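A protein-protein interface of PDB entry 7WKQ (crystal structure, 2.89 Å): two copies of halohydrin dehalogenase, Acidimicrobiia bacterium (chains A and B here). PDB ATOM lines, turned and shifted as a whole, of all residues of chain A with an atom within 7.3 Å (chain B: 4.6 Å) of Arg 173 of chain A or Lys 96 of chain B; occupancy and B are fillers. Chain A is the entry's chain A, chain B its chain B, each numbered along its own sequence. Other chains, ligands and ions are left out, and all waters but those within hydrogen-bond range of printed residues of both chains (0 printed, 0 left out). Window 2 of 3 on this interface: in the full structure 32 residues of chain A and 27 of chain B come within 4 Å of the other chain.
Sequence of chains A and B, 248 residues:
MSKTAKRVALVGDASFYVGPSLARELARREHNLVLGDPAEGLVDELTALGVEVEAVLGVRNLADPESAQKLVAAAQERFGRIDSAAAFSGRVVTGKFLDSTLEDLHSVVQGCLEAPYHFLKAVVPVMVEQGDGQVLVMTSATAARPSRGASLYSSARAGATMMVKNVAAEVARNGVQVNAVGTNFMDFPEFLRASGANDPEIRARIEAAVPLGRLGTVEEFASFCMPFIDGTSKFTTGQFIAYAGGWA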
ATOM      1  N   TYR A 117      16.122  -6.084 -27.031  1.00  0.00           N
ATOM      2  CA  TYR A 117      16.463  -4.731 -26.557  1.00  0.00           C
ATOM      3  C   TYR A 117      15.193  -3.899 -26.525  1.00  0.00           C
ATOM      4  O   TYR A 117      14.908  -3.304 -25.499  1.00  0.00           O
ATOM      5  CB  TYR A 117      17.420  -4.103 -27.569  1.00  0.00           C
ATOM      6  CG  TYR A 117      17.837  -2.682 -27.316  1.00  0.00           C
ATOM      7  CD1 TYR A 117      18.900  -2.398 -26.482  1.00  0.00           C
ATOM      8  CD2 TYR A 117      17.202  -1.625 -27.943  1.00  0.00           C
ATOM      9  CE1 TYR A 117      19.301  -1.097 -26.244  1.00  0.00           C
ATOM     10  CE2 TYR A 117      17.593  -0.318 -27.720  1.00  0.00           C
ATOM     11  CZ  TYR A 117      18.648  -0.055 -26.868  1.00  0.00           C
ATOM     12  OH  TYR A 117      19.047   1.223 -26.635  1.00  0.00           O
ATOM     13  N   LYS A 121      13.618  -2.431 -23.184  1.00  0.00           N
ATOM     14  CA  LYS A 121      13.717  -0.958 -23.118  1.00  0.00           C
ATOM     15  C   LYS A 121      12.350  -0.348 -22.855  1.00  0.00           C
ATOM     16  O   LYS A 121      12.303   0.810 -22.445  1.00  0.00           O
ATOM     17  CB  LYS A 121      14.325  -0.405 -24.402  1.00  0.00           C
ATOM     18  CG  LYS A 121      15.845  -0.371 -24.432  1.00  0.00           C
ATOM     19  CD  LYS A 121      16.451   0.583 -23.430  1.00  0.00           C
ATOM     20  CE  LYS A 121      16.196   2.035 -23.764  1.00  0.00           C
ATOM     21  NZ  LYS A 121      16.696   2.374 -25.114  1.00  0.00           N
ATOM     22  N   GLY A 131       8.689  -0.155  -8.982  1.00  0.00           N
ATOM     23  CA  GLY A 131       9.488  -0.892  -8.019  1.00  0.00           C
ATOM     24  C   GLY A 131       9.193  -2.372  -7.917  1.00  0.00           C
ATOM     25  O   GLY A 131       9.767  -3.046  -7.050  1.00  0.00           O
ATOM     26  N   ALA A 168      19.482  -7.868 -16.171  1.00  0.00           N
ATOM     27  CA  ALA A 168      19.006  -8.478 -14.945  1.00  0.00           C
ATOM     28  C   ALA A 168      19.777  -7.907 -13.768  1.00  0.00           C
ATOM     29  O   ALA A 168      19.191  -7.531 -12.736  1.00  0.00           O
ATOM     30  CB  ALA A 168      19.152  -9.991 -15.039  1.00  0.00           C
ATOM     31  N   ALA A 169      21.089  -7.753 -13.955  1.00  0.00           N
ATOM     32  CA  ALA A 169      21.947  -7.203 -12.911  1.00  0.00           C
ATOM     33  C   ALA A 169      21.628  -5.738 -12.592  1.00  0.00           C
ATOM     34  O   ALA A 169      21.537  -5.372 -11.413  1.00  0.00           O
ATOM     35  CB  ALA A 169      23.416  -7.362 -13.312  1.00  0.00           C
ATOM     36  N   GLU A 170      21.492  -4.880 -13.615  1.00  0.00           N
ATOM     37  CA  GLU A 170      21.203  -3.458 -13.373  1.00  0.00           C
ATOM     38  C   GLU A 170      19.945  -3.274 -12.540  1.00  0.00           C
ATOM     39  O   GLU A 170      19.940  -2.550 -11.534  1.00  0.00           O
ATOM     40  CB  GLU A 170      21.021  -2.679 -14.677  1.00  0.00           C
ATOM     41  CG  GLU A 170      22.277  -2.422 -15.449  1.00  0.00           C
ATOM     42  CD  GLU A 170      22.019  -1.648 -16.727  1.00  0.00           C
ATOM     43  OE1 GLU A 170      22.667  -1.991 -17.738  1.00  0.00           O
ATOM     44  OE2 GLU A 170      21.184  -0.711 -16.728  1.00  0.00           O
ATOM     45  N   VAL A 171      18.861  -3.943 -12.933  1.00  0.00           N
ATOM     46  CA  VAL A 171      17.572  -3.590 -12.353  1.00  0.00           C
ATOM     47  C   VAL A 171      17.192  -4.492 -11.194  1.00  0.00           C
ATOM     48  O   VAL A 171      16.098  -4.328 -10.629  1.00  0.00           O
ATOM     49  CB  VAL A 171      16.484  -3.602 -13.443  1.00  0.00           C
ATOM     50  CG1 VAL A 171      16.828  -2.572 -14.511  1.00  0.00           C
ATOM     51  CG2 VAL A 171      16.343  -4.990 -14.038  1.00  0.00           C
ATOM     52  N   ALA A 172      18.058  -5.450 -10.821  1.00  0.00           N
ATOM     53  CA  ALA A 172      17.780  -6.239  -9.625  1.00  0.00           C
ATOM     54  C   ALA A 172      17.494  -5.357  -8.408  1.00  0.00           C
ATOM     55  O   ALA A 172      16.528  -5.596  -7.669  1.00  0.00           O
ATOM     56  CB  ALA A 172      18.926  -7.205  -9.354  1.00  0.00           C
ATOM     57  N   ARG A 173      18.297  -4.321  -8.188  1.00  0.00           N
ATOM     58  CA  ARG A 173      18.032  -3.445  -7.048  1.00  0.00           C
ATOM     59  C   ARG A 173      16.665  -2.768  -7.108  1.00  0.00           C
ATOM     60  O   ARG A 173      16.080  -2.482  -6.055  1.00  0.00           O
ATOM     61  CB  ARG A 173      19.140  -2.403  -6.896  1.00  0.00           C
ATOM     62  CG  ARG A 173      19.291  -1.517  -8.094  1.00  0.00           C
ATOM     63  CD  ARG A 173      20.012  -0.246  -7.739  1.00  0.00           C
ATOM     64  NE  ARG A 173      19.958   0.699  -8.846  1.00  0.00           N
ATOM     65  CZ  ARG A 173      20.774   1.740  -8.988  1.00  0.00           C
ATOM     66  NH1 ARG A 173      21.740   1.969  -8.094  1.00  0.00           N
ATOM     67  NH2 ARG A 173      20.625   2.549 -10.035  1.00  0.00           N
ATOM     68  N   ASN A 174      16.132  -2.494  -8.300  1.00  0.00           N
ATOM     69  CA  ASN A 174      14.928  -1.681  -8.324  1.00  0.00           C
ATOM     70  C   ASN A 174      13.694  -2.540  -8.156  1.00  0.00           C
ATOM     71  O   ASN A 174      12.581  -2.043  -8.351  1.00  0.00           O
ATOM     72  CB  ASN A 174      14.773  -0.892  -9.622  1.00  0.00           C
ATOM     73  CG  ASN A 174      16.004  -0.113  -9.996  1.00  0.00           C
ATOM     74  OD1 ASN A 174      16.826   0.217  -9.149  1.00  0.00           O
ATOM     75  ND2 ASN A 174      16.038   0.329 -11.243  1.00  0.00           N
ATOM     76  N   GLY A 175      13.888  -3.820  -7.825  1.00  0.00           N
ATOM     77  CA  GLY A 175      12.823  -4.765  -7.581  1.00  0.00           C
ATOM     78  C   GLY A 175      12.322  -5.481  -8.807  1.00  0.00           C
ATOM     79  O   GLY A 175      11.261  -6.122  -8.743  1.00  0.00           O
ATOM     80  N   VAL A 176      13.049  -5.382  -9.926  1.00  0.00           N
ATOM     81  CA  VAL A 176      12.647  -5.989 -11.191  1.00  0.00           C
ATOM     82  C   VAL A 176      13.527  -7.207 -11.459  1.00  0.00           C
ATOM     83  O   VAL A 176      14.752  -7.085 -11.603  1.00  0.00           O
ATOM     84  CB  VAL A 176      12.747  -4.992 -12.350  1.00  0.00           C
ATOM     85  CG1 VAL A 176      12.218  -5.649 -13.588  1.00  0.00           C
ATOM     86  CG2 VAL A 176      12.049  -3.670 -12.004  1.00  0.00           C
ATOM     87  N   THR A 237      16.530 -13.887 -10.025  1.00  0.00           N
ATOM     88  CA  THR A 237      16.785 -12.933 -11.098  1.00  0.00           C
ATOM     89  C   THR A 237      18.058 -13.384 -11.797  1.00  0.00           C
ATOM     90  O   THR A 237      18.886 -14.092 -11.218  1.00  0.00           O
ATOM     91  CB  THR A 237      16.961 -11.481 -10.616  1.00  0.00           C
ATOM     92  OG1 THR A 237      16.848 -10.565 -11.718  1.00  0.00           O
ATOM     93  CG2 THR A 237      18.373 -11.320 -10.089  1.00  0.00           C
ATOM     94  N   GLY B  95      27.314   3.434 -20.807  1.00  0.00           N
ATOM     95  CA  GLY B  95      26.047   3.881 -20.259  1.00  0.00           C
ATOM     96  C   GLY B  95      25.298   2.641 -19.806  1.00  0.00           C
ATOM     97  O   GLY B  95      25.430   1.556 -20.379  1.00  0.00           O
ATOM     98  N   LYS B  96      24.524   2.793 -18.736  1.00  0.00           N
ATOM     99  CA  LYS B  96      23.582   1.757 -18.340  1.00  0.00           C
ATOM    100  C   LYS B  96      22.641   1.463 -19.501  1.00  0.00           C
ATOM    101  O   LYS B  96      22.381   2.319 -20.350  1.00  0.00           O
ATOM    102  CB  LYS B  96      22.762   2.191 -17.141  1.00  0.00           C
ATOM    103  CG  LYS B  96      23.494   2.311 -15.818  1.00  0.00           C
ATOM    104  CD  LYS B  96      22.438   2.899 -14.901  1.00  0.00           C
ATOM    105  CE  LYS B  96      22.903   3.261 -13.514  1.00  0.00           C
ATOM    106  NZ  LYS B  96      21.787   3.934 -12.729  1.00  0.00           N
ATOM    107  N   PHE B  97      22.133   0.232 -19.520  1.00  0.00           N
ATOM    108  CA  PHE B  97      21.251  -0.246 -20.581  1.00  0.00           C
ATOM    109  C   PHE B  97      20.091   0.707 -20.825  1.00  0.00           C
ATOM    110  O   PHE B  97      19.868   1.157 -21.958  1.00  0.00           O
ATOM    111  CB  PHE B  97      20.713  -1.620 -20.191  1.00  0.00           C
ATOM    112  CG  PHE B  97      19.670  -2.149 -21.104  1.00  0.00           C
ATOM    113  CD1 PHE B  97      18.390  -2.416 -20.620  1.00  0.00           C
ATOM    114  CD2 PHE B  97      19.974  -2.447 -22.420  1.00  0.00           C
ATOM    115  CE1 PHE B  97      17.417  -2.941 -21.440  1.00  0.00           C
ATOM    116  CE2 PHE B  97      18.995  -2.982 -23.274  1.00  0.00           C
ATOM    117  CZ  PHE B  97      17.712  -3.225 -22.783  1.00  0.00           C
ATOM    118  N   LEU B  98      19.317   1.000 -19.764  1.00  0.00           N
ATOM    119  CA  LEU B  98      18.088   1.785 -19.887  1.00  0.00           C
ATOM    120  C   LEU B  98      18.336   3.189 -20.400  1.00  0.00           C
ATOM    121  O   LEU B  98      17.387   3.879 -20.787  1.00  0.00           O
ATOM    122  CB  LEU B  98      17.379   1.814 -18.545  1.00  0.00           C
ATOM    123  CG  LEU B  98      16.925   0.439 -18.078  1.00  0.00           C
ATOM    124  CD1 LEU B  98      16.326   0.523 -16.688  1.00  0.00           C
ATOM    125  CD2 LEU B  98      15.916  -0.141 -19.054  1.00  0.00           C
ATOM    126  N   ASP B  99      19.597   3.616 -20.432  1.00  0.00           N
ATOM    127  CA  ASP B  99      19.979   4.945 -20.882  1.00  0.00           C
ATOM    128  C   ASP B  99      20.535   4.976 -22.301  1.00  0.00           C
ATOM    129  O   ASP B  99      20.666   6.061 -22.874  1.00  0.00           O
ATOM    130  CB  ASP B  99      21.017   5.507 -19.905  1.00  0.00           C
ATOM    131  CG  ASP B  99      20.416   5.901 -18.552  1.00  0.00           C
ATOM    132  OD1 ASP B  99      19.334   5.403 -18.153  1.00  0.00           O
ATOM    133  OD2 ASP B  99      21.095   6.664 -17.841  1.00  0.00           O
ATOM    134  N   SER B 100      20.741   3.789 -22.859  1.00  0.00           N
ATOM    135  CA  SER B 100      21.311   3.659 -24.215  1.00  0.00           C
ATOM    136  C   SER B 100      20.281   3.961 -25.288  1.00  0.00           C
ATOM    137  O   SER B 100      19.110   4.154 -24.952  1.00  0.00           O
ATOM    138  CB  SER B 100      21.802   2.272 -24.398  1.00  0.00           C
ATOM    139  OG  SER B 100      20.718   1.362 -24.438  1.00  0.00           O
ATOM    140  N   GLY B 149      27.423  -0.717 -16.281  1.00  0.00           N
ATOM    141  CA  GLY B 149      28.701  -0.145 -16.745  1.00  0.00           C
ATOM    142  C   GLY B 149      28.739   0.048 -18.251  1.00  0.00           C
ATOM    143  O   GLY B 149      28.810   1.205 -18.687  1.00  0.00           O
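The side-chain hydroxyl of Tyr 117 of chain A is in hydrogen-bond range of the side-chain amino group of Lys 121 of chain A (3.0 Å).
The backbone NH (N) of Val 176 of chain A lies within hydrogen-bond range of the backbone carbonyl oxygen (O) of Val 171 of chain A, 3.3 Å away.
OD1 of Asn 174 of chain A is in hydrogen-bond range of NE of Arg 173 of chain A, 3.2 Å away.
The backbone carbonyl oxygen of Phe 97 of chain B lies within hydrogen-bond range of the side-chain hydroxyl of Ser 100 of chain B, 2.6 Å away.
Of chain B, only Lys 96 comes within 4 Å of Arg 173 of chain A.
Of chain A, only Glu 170 and Arg 173 come within 4 Å of Lys 96 of chain B.
Of the printed residues of chain B, Val 171 of chain A touches Leu 98.
Printed residues of chain A within 4 Å of Leu 98 of chain B: Lys 121 (3.7 Å), Glu 170 (3.95 Å) and Val 171 (3.8 Å).
Of the printed residues of chain B, Tyr 117 of chain A touches Phe 97 (3.3 Å) and Ser 100 (2.8 Å).
Of the printed residues of chain B, Glu 170 of chain A touches Lys 96, Phe 97 and Leu 98.
Of the printed residues of chain A, Phe 97 of chain B touches Tyr 117 (3.3 Å), Lys 121 (3.8 Å) and Glu 170 (2.9 Å).
Thr 237 of chain A touches none of the printed residues of chain B.
The nearest residue of chain A that does not touch Lys 96 of chain B is Lys 121 of chain A (6.9 Å).
The nearest printed residue of chain A that does not touch Leu 98 of chain B is Asn 174 of chain A (5.5 Å).
No position is printed for both chains.
Of the 10 pairs that touch across the chains among the printed residues, none has its exchanged pair printed and touching as well.
OH of Tyr 117 of chain A sits at hydrogen-bond distance from OG of Ser 100 of chain B, 2.8 Å away.
The side-chain amino group of Lys 121 of chain A is in hydrogen-bond range of the backbone carbonyl oxygen of Ser 100 of chain B, at 3.0 Å.
OE1 of Glu 170 of chain A lies within hydrogen-bond range of N of Phe 97 of chain B, 2.9 Å away.
The guanidinium group (NH2) of Arg 173 of chain A sits close to the side-chain amino group (NZ) of Lys 96 of chain B.
Of the 13 printed residues of chain A, 5 touch a printed residue of chain B.
Printed residues of chain A that touch a printed residue of chain B: Tyr 117, Lys 121, Glu 170, Val 171 and Arg 173.
Hydrophobic or aromatic side chains of chain A that line the printed part of chain B: Tyr 117 and Val 171.
Of the 7 printed residues of chain B, 4 touch a printed residue of chain A.
Among the printed residues, 10 pairs touch across the chains.
Among the printed residues, no Asp or Glu carboxylate lies within 4 Å of a Lys or Arg side-chain nitrogen of the other chain.
CE2 of Phe 97 of chain B touches CD1 of Tyr 117 of chain A, at 3.3 Å.
Lys 121 of chain A touches Phe 97 of chain B.
CE of Lys 121 of chain A touches O of Leu 98 of chain B, 3.7 Å away.
Glu 170 of chain A touches Lys 96 of chain B.
OE2 of Glu 170 of chain A touches N of Leu 98 of chain B, at 3.95 Å.
CG1 of Val 171 of chain A touches CD1 of Leu 98 of chain B, at 3.8 Å.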
